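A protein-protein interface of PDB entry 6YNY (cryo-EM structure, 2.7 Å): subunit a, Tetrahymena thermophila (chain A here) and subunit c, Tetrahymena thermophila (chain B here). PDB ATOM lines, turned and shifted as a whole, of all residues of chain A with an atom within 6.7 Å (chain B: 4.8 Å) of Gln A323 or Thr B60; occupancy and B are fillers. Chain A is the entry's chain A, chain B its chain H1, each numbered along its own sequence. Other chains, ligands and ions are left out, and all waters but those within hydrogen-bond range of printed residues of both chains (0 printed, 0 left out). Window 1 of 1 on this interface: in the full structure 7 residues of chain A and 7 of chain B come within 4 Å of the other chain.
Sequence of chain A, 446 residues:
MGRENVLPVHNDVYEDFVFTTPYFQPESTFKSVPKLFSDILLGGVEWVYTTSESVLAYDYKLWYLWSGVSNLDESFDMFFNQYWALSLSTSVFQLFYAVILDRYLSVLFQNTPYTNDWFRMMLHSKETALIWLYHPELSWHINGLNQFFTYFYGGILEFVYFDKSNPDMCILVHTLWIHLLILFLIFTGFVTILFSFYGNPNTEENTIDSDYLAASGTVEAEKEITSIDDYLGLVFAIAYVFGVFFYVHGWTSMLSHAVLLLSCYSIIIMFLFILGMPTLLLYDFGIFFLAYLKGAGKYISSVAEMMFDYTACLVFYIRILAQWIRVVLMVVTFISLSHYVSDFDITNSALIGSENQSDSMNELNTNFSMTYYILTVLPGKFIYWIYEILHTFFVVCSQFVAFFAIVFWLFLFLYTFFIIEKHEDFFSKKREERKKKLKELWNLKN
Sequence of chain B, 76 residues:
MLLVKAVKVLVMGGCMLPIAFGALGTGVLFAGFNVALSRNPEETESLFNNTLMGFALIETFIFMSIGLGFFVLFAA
Of the printed residues of chain B, Gln A323 touches Thr B60.
Thr B60 touches just one residue of chain A: Gln A323 (3.9 Å).
Printed residues of chain A within 4 Å of Met B64: Ile A318 (3.96 Å).
Printed residues of chain A within 4 Å of Glu B59: Arg A326 (2.5 Å).
Of the printed residues of chain B, Ile A406 touches Ala B56 (3.5 Å).
The nearest printed residue of chain B that does not touch Gln A323 is Phe B63 (4.8 Å).
Among the printed residues, pairs that only touch across the chains: Arg A326 with Phe B63 (3.4 Å), Ile A406 with Ala B56 (3.5 Å), Ile A325 with Phe B63 (3.6 Å), Ala A322 with Phe B63 (3.7 Å), Gln A323 with Thr B60 (3.9 Å) and Ile A318 with Met B64 (3.96 Å).
OE1 of Glu B59 lies within salt-bridge range of NH2 of Arg A326, at 2.5 Å.
Hydrophobic or aromatic side chains of chain B within 4 Å of the printed part of chain A: Ala B56, Phe B63 and Met B64.
Of the 16 printed residues of chain A, 6 touch a printed residue of chain B.
Hydrophobic or aromatic side chains of chain A that line the printed part of chain B: Ile A318, Ile A325 and Ile A406.
Along chain A the printed residues that touch a printed residue of chain B span positions 318 to 406.
Among the printed residues, 7 pairs touch across the chains.
Among the printed residues, Asp or Glu carboxylates within 4 Å of a Lys or Arg side-chain nitrogen of the other chain: Arg A326 with Glu B59.
OE1 of Gln A399 lies within hydrogen-bond range of NH2 of Arg A326.
The side-chain amide oxygen of Gln A323 sits close to the guanidinium group of Arg A326, 3.2 Å away.
O of Ala B56 is in hydrogen-bond range of OG1 of Thr B60 (2.5 Å).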
ATOM      1  N   ILE A 318      15.071 -15.106   6.608  1.00  0.00           N
ATOM      2  CA  ILE A 318      14.317 -16.342   6.778  1.00  0.00           C
ATOM      3  C   ILE A 318      14.527 -16.912   8.171  1.00  0.00           C
ATOM      4  O   ILE A 318      13.611 -17.508   8.749  1.00  0.00           O
ATOM      5  CB  ILE A 318      14.705 -17.354   5.688  1.00  0.00           C
ATOM      6  CG1 ILE A 318      14.318 -16.821   4.307  1.00  0.00           C
ATOM      7  CG2 ILE A 318      14.045 -18.686   5.943  1.00  0.00           C
ATOM      8  CD1 ILE A 318      12.858 -16.466   4.160  1.00  0.00           C
ATOM      9  N   ARG A 319      15.724 -16.750   8.733  1.00  0.00           N
ATOM     10  CA  ARG A 319      15.956 -17.153  10.113  1.00  0.00           C
ATOM     11  C   ARG A 319      14.968 -16.500  11.067  1.00  0.00           C
ATOM     12  O   ARG A 319      14.716 -17.039  12.149  1.00  0.00           O
ATOM     13  CB  ARG A 319      17.378 -16.795  10.541  1.00  0.00           C
ATOM     14  CG  ARG A 319      18.471 -17.521   9.791  1.00  0.00           C
ATOM     15  CD  ARG A 319      19.830 -17.043  10.250  1.00  0.00           C
ATOM     16  NE  ARG A 319      20.912 -17.506   9.389  1.00  0.00           N
ATOM     17  CZ  ARG A 319      21.489 -18.697   9.487  1.00  0.00           C
ATOM     18  NH1 ARG A 319      21.087 -19.560  10.408  1.00  0.00           N
ATOM     19  NH2 ARG A 319      22.470 -19.026   8.659  1.00  0.00           N
ATOM     20  N   ILE A 320      14.413 -15.352  10.691  1.00  0.00           N
ATOM     21  CA  ILE A 320      13.464 -14.622  11.519  1.00  0.00           C
ATOM     22  C   ILE A 320      12.037 -14.995  11.152  1.00  0.00           C
ATOM     23  O   ILE A 320      11.270 -15.471  11.996  1.00  0.00           O
ATOM     24  CB  ILE A 320      13.682 -13.107  11.372  1.00  0.00           C
ATOM     25  CG1 ILE A 320      15.092 -12.722  11.814  1.00  0.00           C
ATOM     26  CG2 ILE A 320      12.646 -12.339  12.165  1.00  0.00           C
ATOM     27  CD1 ILE A 320      15.337 -12.888  13.280  1.00  0.00           C
ATOM     28  N   LEU A 321      11.670 -14.787   9.887  1.00  0.00           N
ATOM     29  CA  LEU A 321      10.290 -15.014   9.479  1.00  0.00           C
ATOM     30  C   LEU A 321       9.878 -16.468   9.648  1.00  0.00           C
ATOM     31  O   LEU A 321       8.702 -16.754   9.891  1.00  0.00           O
ATOM     32  CB  LEU A 321      10.098 -14.578   8.029  1.00  0.00           C
ATOM     33  CG  LEU A 321      10.505 -13.139   7.713  1.00  0.00           C
ATOM     34  CD1 LEU A 321      10.184 -12.811   6.269  1.00  0.00           C
ATOM     35  CD2 LEU A 321       9.823 -12.161   8.644  1.00  0.00           C
ATOM     36  N   ALA A 322      10.822 -17.398   9.522  1.00  0.00           N
ATOM     37  CA  ALA A 322      10.488 -18.808   9.664  1.00  0.00           C
ATOM     38  C   ALA A 322      10.074 -19.166  11.083  1.00  0.00           C
ATOM     39  O   ALA A 322       9.391 -20.174  11.280  1.00  0.00           O
ATOM     40  CB  ALA A 322      11.672 -19.673   9.241  1.00  0.00           C
ATOM     41  N   GLN A 323      10.468 -18.365  12.071  1.00  0.00           N
ATOM     42  CA  GLN A 323      10.115 -18.639  13.456  1.00  0.00           C
ATOM     43  C   GLN A 323       8.679 -18.267  13.786  1.00  0.00           C
ATOM     44  O   GLN A 323       8.202 -18.616  14.870  1.00  0.00           O
ATOM     45  CB  GLN A 323      11.070 -17.896  14.389  1.00  0.00           C
ATOM     46  CG  GLN A 323      12.521 -18.215  14.137  1.00  0.00           C
ATOM     47  CD  GLN A 323      12.814 -19.692  14.234  1.00  0.00           C
ATOM     48  OE1 GLN A 323      12.297 -20.382  15.109  1.00  0.00           O
ATOM     49  NE2 GLN A 323      13.637 -20.190  13.326  1.00  0.00           N
ATOM     50  N   TRP A 324       7.983 -17.574  12.888  1.00  0.00           N
ATOM     51  CA  TRP A 324       6.574 -17.283  13.087  1.00  0.00           C
ATOM     52  C   TRP A 324       5.686 -18.481  12.792  1.00  0.00           C
ATOM     53  O   TRP A 324       4.502 -18.455  13.141  1.00  0.00           O
ATOM     54  CB  TRP A 324       6.155 -16.099  12.219  1.00  0.00           C
ATOM     55  CG  TRP A 324       6.624 -14.798  12.770  1.00  0.00           C
ATOM     56  CD1 TRP A 324       7.722 -14.094  12.389  1.00  0.00           C
ATOM     57  CD2 TRP A 324       6.009 -14.047  13.819  1.00  0.00           C
ATOM     58  NE1 TRP A 324       7.831 -12.948  13.133  1.00  0.00           N
ATOM     59  CE2 TRP A 324       6.789 -12.895  14.019  1.00  0.00           C
ATOM     60  CE3 TRP A 324       4.873 -14.236  14.608  1.00  0.00           C
ATOM     61  CZ2 TRP A 324       6.471 -11.937  14.973  1.00  0.00           C
ATOM     62  CZ3 TRP A 324       4.559 -13.283  15.553  1.00  0.00           C
ATOM     63  CH2 TRP A 324       5.353 -12.150  15.729  1.00  0.00           C
ATOM     64  N   ILE A 325       6.226 -19.520  12.158  1.00  0.00           N
ATOM     65  CA  ILE A 325       5.477 -20.759  12.015  1.00  0.00           C
ATOM     66  C   ILE A 325       5.313 -21.428  13.369  1.00  0.00           C
ATOM     67  O   ILE A 325       4.348 -22.166  13.594  1.00  0.00           O
ATOM     68  CB  ILE A 325       6.172 -21.685  11.003  1.00  0.00           C
ATOM     69  CG1 ILE A 325       6.264 -20.993   9.643  1.00  0.00           C
ATOM     70  CG2 ILE A 325       5.428 -22.999  10.887  1.00  0.00           C
ATOM     71  CD1 ILE A 325       6.964 -21.803   8.590  1.00  0.00           C
ATOM     72  N   ARG A 326       6.247 -21.187  14.289  1.00  0.00           N
ATOM     73  CA  ARG A 326       6.083 -21.681  15.649  1.00  0.00           C
ATOM     74  C   ARG A 326       4.870 -21.050  16.314  1.00  0.00           C
ATOM     75  O   ARG A 326       4.135 -21.718  17.048  1.00  0.00           O
ATOM     76  CB  ARG A 326       7.344 -21.397  16.461  1.00  0.00           C
ATOM     77  CG  ARG A 326       8.602 -21.996  15.887  1.00  0.00           C
ATOM     78  CD  ARG A 326       9.798 -21.659  16.741  1.00  0.00           C
ATOM     79  NE  ARG A 326      11.048 -22.077  16.119  1.00  0.00           N
ATOM     80  CZ  ARG A 326      11.601 -23.274  16.273  1.00  0.00           C
ATOM     81  NH1 ARG A 326      12.740 -23.553  15.663  1.00  0.00           N
ATOM     82  NH2 ARG A 326      11.021 -24.197  17.023  1.00  0.00           N
ATOM     83  N   VAL A 327       4.647 -19.758  16.068  1.00  0.00           N
ATOM     84  CA  VAL A 327       3.496 -19.074  16.641  1.00  0.00           C
ATOM     85  C   VAL A 327       2.203 -19.651  16.092  1.00  0.00           C
ATOM     86  O   VAL A 327       1.197 -19.731  16.806  1.00  0.00           O
ATOM     87  CB  VAL A 327       3.600 -17.562  16.375  1.00  0.00           C
ATOM     88  CG1 VAL A 327       2.406 -16.842  16.945  1.00  0.00           C
ATOM     89  CG2 VAL A 327       4.879 -17.013  16.966  1.00  0.00           C
ATOM     90  N   VAL A 328       2.200 -20.061  14.824  1.00  0.00           N
ATOM     91  CA  VAL A 328       1.010 -20.669  14.243  1.00  0.00           C
ATOM     92  C   VAL A 328       0.687 -21.980  14.947  1.00  0.00           C
ATOM     93  O   VAL A 328      -0.477 -22.278  15.237  1.00  0.00           O
ATOM     94  CB  VAL A 328       1.200 -20.872  12.730  1.00  0.00           C
ATOM     95  CG1 VAL A 328       0.006 -21.569  12.140  1.00  0.00           C
ATOM     96  CG2 VAL A 328       1.416 -19.544  12.041  1.00  0.00           C
ATOM     97  N   GLN A 399       7.773 -24.140  21.903  1.00  0.00           N
ATOM     98  CA  GLN A 399       7.871 -23.201  20.793  1.00  0.00           C
ATOM     99  C   GLN A 399       8.013 -21.766  21.278  1.00  0.00           C
ATOM    100  O   GLN A 399       8.589 -20.930  20.574  1.00  0.00           O
ATOM    101  CB  GLN A 399       6.651 -23.341  19.890  1.00  0.00           C
ATOM    102  CG  GLN A 399       6.532 -24.696  19.235  1.00  0.00           C
ATOM    103  CD  GLN A 399       7.755 -25.070  18.439  1.00  0.00           C
ATOM    104  OE1 GLN A 399       8.487 -24.209  17.955  1.00  0.00           O
ATOM    105  NE2 GLN A 399       7.993 -26.366  18.306  1.00  0.00           N
ATOM    106  N   ALA A 402      11.778 -21.505  21.967  1.00  0.00           N
ATOM    107  CA  ALA A 402      12.534 -21.577  20.724  1.00  0.00           C
ATOM    108  C   ALA A 402      12.405 -20.297  19.914  1.00  0.00           C
ATOM    109  O   ALA A 402      13.312 -19.953  19.150  1.00  0.00           O
ATOM    110  CB  ALA A 402      12.065 -22.772  19.902  1.00  0.00           C
ATOM    111  N   PHE A 403      11.295 -19.580  20.069  1.00  0.00           N
ATOM    112  CA  PHE A 403      11.093 -18.358  19.301  1.00  0.00           C
ATOM    113  C   PHE A 403      12.064 -17.269  19.737  1.00  0.00           C
ATOM    114  O   PHE A 403      12.781 -16.695  18.910  1.00  0.00           O
ATOM    115  CB  PHE A 403       9.649 -17.885  19.450  1.00  0.00           C
ATOM    116  CG  PHE A 403       9.349 -16.620  18.709  1.00  0.00           C
ATOM    117  CD1 PHE A 403       9.481 -15.393  19.327  1.00  0.00           C
ATOM    118  CD2 PHE A 403       8.941 -16.657  17.394  1.00  0.00           C
ATOM    119  CE1 PHE A 403       9.210 -14.232  18.645  1.00  0.00           C
ATOM    120  CE2 PHE A 403       8.670 -15.499  16.710  1.00  0.00           C
ATOM    121  CZ  PHE A 403       8.805 -14.286  17.338  1.00  0.00           C
ATOM    122  N   ILE A 406      15.928 -17.957  19.455  1.00  0.00           N
ATOM    123  CA  ILE A 406      16.455 -17.954  18.102  1.00  0.00           C
ATOM    124  C   ILE A 406      16.359 -16.575  17.466  1.00  0.00           C
ATOM    125  O   ILE A 406      17.313 -16.107  16.844  1.00  0.00           O
ATOM    126  CB  ILE A 406      15.731 -19.009  17.238  1.00  0.00           C
ATOM    127  CG1 ILE A 406      15.915 -20.401  17.836  1.00  0.00           C
ATOM    128  CG2 ILE A 406      16.247 -18.969  15.818  1.00  0.00           C
ATOM    129  CD1 ILE A 406      15.040 -21.453  17.212  1.00  0.00           C
ATOM    130  N   VAL A 407      15.215 -15.908  17.618  1.00  0.00           N
ATOM    131  CA  VAL A 407      15.008 -14.622  16.967  1.00  0.00           C
ATOM    132  C   VAL A 407      15.894 -13.548  17.578  1.00  0.00           C
ATOM    133  O   VAL A 407      16.332 -12.626  16.881  1.00  0.00           O
ATOM    134  CB  VAL A 407      13.522 -14.238  17.036  1.00  0.00           C
ATOM    135  CG1 VAL A 407      13.326 -12.788  16.667  1.00  0.00           C
ATOM    136  CG2 VAL A 407      12.719 -15.122  16.120  1.00  0.00           C
ATOM    137  N   ALA B  56      17.875 -26.284  16.610  1.00  0.00           N
ATOM    138  CA  ALA B  56      17.152 -25.138  16.077  1.00  0.00           C
ATOM    139  C   ALA B  56      17.387 -25.004  14.581  1.00  0.00           C
ATOM    140  O   ALA B  56      16.438 -24.919  13.794  1.00  0.00           O
ATOM    141  CB  ALA B  56      17.581 -23.868  16.808  1.00  0.00           C
ATOM    142  N   LEU B  57      18.656 -24.994  14.170  1.00  0.00           N
ATOM    143  CA  LEU B  57      18.969 -24.897  12.749  1.00  0.00           C
ATOM    144  C   LEU B  57      18.367 -26.057  11.971  1.00  0.00           C
ATOM    145  O   LEU B  57      18.058 -25.914  10.783  1.00  0.00           O
ATOM    146  CB  LEU B  57      20.483 -24.853  12.549  1.00  0.00           C
ATOM    147  CG  LEU B  57      21.169 -23.516  12.827  1.00  0.00           C
ATOM    148  CD1 LEU B  57      20.828 -23.001  14.210  1.00  0.00           C
ATOM    149  CD2 LEU B  57      22.666 -23.665  12.678  1.00  0.00           C
ATOM    150  N   ILE B  58      18.191 -27.209  12.619  1.00  0.00           N
ATOM    151  CA  ILE B  58      17.662 -28.381  11.930  1.00  0.00           C
ATOM    152  C   ILE B  58      16.204 -28.156  11.549  1.00  0.00           C
ATOM    153  O   ILE B  58      15.841 -28.194  10.367  1.00  0.00           O
ATOM    154  CB  ILE B  58      17.842 -29.637  12.799  1.00  0.00           C
ATOM    155  CG1 ILE B  58      19.306 -30.088  12.743  1.00  0.00           C
ATOM    156  CG2 ILE B  58      16.891 -30.743  12.365  1.00  0.00           C
ATOM    157  CD1 ILE B  58      19.649 -31.200  13.696  1.00  0.00           C
ATOM    158  N   GLU B  59      15.343 -27.920  12.541  1.00  0.00           N
ATOM    159  CA  GLU B  59      13.942 -27.663  12.231  1.00  0.00           C
ATOM    160  C   GLU B  59      13.747 -26.346  11.494  1.00  0.00           C
ATOM    161  O   GLU B  59      12.665 -26.120  10.942  1.00  0.00           O
ATOM    162  CB  GLU B  59      13.091 -27.677  13.501  1.00  0.00           C
ATOM    163  CG  GLU B  59      13.512 -26.691  14.560  1.00  0.00           C
ATOM    164  CD  GLU B  59      12.630 -26.773  15.788  1.00  0.00           C
ATOM    165  OE1 GLU B  59      12.780 -25.923  16.690  1.00  0.00           O
ATOM    166  OE2 GLU B  59      11.783 -27.689  15.850  1.00  0.00           O
ATOM    167  N   THR B  60      14.756 -25.476  11.479  1.00  0.00           N
ATOM    168  CA  THR B  60      14.673 -24.262  10.675  1.00  0.00           C
ATOM    169  C   THR B  60      14.493 -24.610   9.203  1.00  0.00           C
ATOM    170  O   THR B  60      13.602 -24.081   8.529  1.00  0.00           O
ATOM    171  CB  THR B  60      15.924 -23.409  10.884  1.00  0.00           C
ATOM    172  OG1 THR B  60      16.026 -23.036  12.263  1.00  0.00           O
ATOM    173  CG2 THR B  60      15.872 -22.157  10.032  1.00  0.00           C
ATOM    174  N   PHE B  61      15.342 -25.503   8.685  1.00  0.00           N
ATOM    175  CA  PHE B  61      15.145 -26.004   7.331  1.00  0.00           C
ATOM    176  C   PHE B  61      13.768 -26.634   7.181  1.00  0.00           C
ATOM    177  O   PHE B  61      13.100 -26.453   6.155  1.00  0.00           O
ATOM    178  CB  PHE B  61      16.227 -27.024   6.982  1.00  0.00           C
ATOM    179  CG  PHE B  61      17.612 -26.452   6.920  1.00  0.00           C
ATOM    180  CD1 PHE B  61      18.057 -25.795   5.785  1.00  0.00           C
ATOM    181  CD2 PHE B  61      18.476 -26.587   7.990  1.00  0.00           C
ATOM    182  CE1 PHE B  61      19.336 -25.275   5.726  1.00  0.00           C
ATOM    183  CE2 PHE B  61      19.755 -26.069   7.937  1.00  0.00           C
ATOM    184  CZ  PHE B  61      20.185 -25.413   6.804  1.00  0.00           C
ATOM    185  N   ILE B  62      13.329 -27.380   8.195  1.00  0.00           N
ATOM    186  CA  ILE B  62      12.023 -28.030   8.133  1.00  0.00           C
ATOM    187  C   ILE B  62      10.927 -26.990   7.953  1.00  0.00           C
ATOM    188  O   ILE B  62      10.063 -27.115   7.077  1.00  0.00           O
ATOM    189  CB  ILE B  62      11.792 -28.879   9.394  1.00  0.00           C
ATOM    190  CG1 ILE B  62      12.911 -29.913   9.557  1.00  0.00           C
ATOM    191  CG2 ILE B  62      10.435 -29.563   9.336  1.00  0.00           C
ATOM    192  CD1 ILE B  62      13.091 -30.826   8.369  1.00  0.00           C
ATOM    193  N   PHE B  63      10.939 -25.948   8.786  1.00  0.00           N
ATOM    194  CA  PHE B  63       9.989 -24.858   8.605  1.00  0.00           C
ATOM    195  C   PHE B  63      10.158 -24.212   7.238  1.00  0.00           C
ATOM    196  O   PHE B  63       9.170 -23.870   6.577  1.00  0.00           O
ATOM    197  CB  PHE B  63      10.161 -23.819   9.714  1.00  0.00           C
ATOM    198  CG  PHE B  63       9.700 -24.283  11.071  1.00  0.00           C
ATOM    199  CD1 PHE B  63       8.749 -25.283  11.205  1.00  0.00           C
ATOM    200  CD2 PHE B  63      10.214 -23.704  12.218  1.00  0.00           C
ATOM    201  CE1 PHE B  63       8.330 -25.698  12.450  1.00  0.00           C
ATOM    202  CE2 PHE B  63       9.796 -24.116  13.467  1.00  0.00           C
ATOM    203  CZ  PHE B  63       8.852 -25.114  13.582  1.00  0.00           C
ATOM    204  N   MET B  64      11.404 -24.038   6.798  1.00  0.00           N
ATOM    205  CA  MET B  64      11.652 -23.457   5.485  1.00  0.00           C
ATOM    206  C   MET B  64      10.967 -24.266   4.391  1.00  0.00           C
ATOM    207  O   MET B  64      10.408 -23.699   3.445  1.00  0.00           O
ATOM    208  CB  MET B  64      13.156 -23.380   5.231  1.00  0.00           C
ATOM    209  CG  MET B  64      13.542 -22.670   3.947  1.00  0.00           C
ATOM    210  SD  MET B  64      15.311 -22.737   3.606  1.00  0.00           S
ATOM    211  CE  MET B  64      15.980 -22.043   5.113  1.00  0.00           C
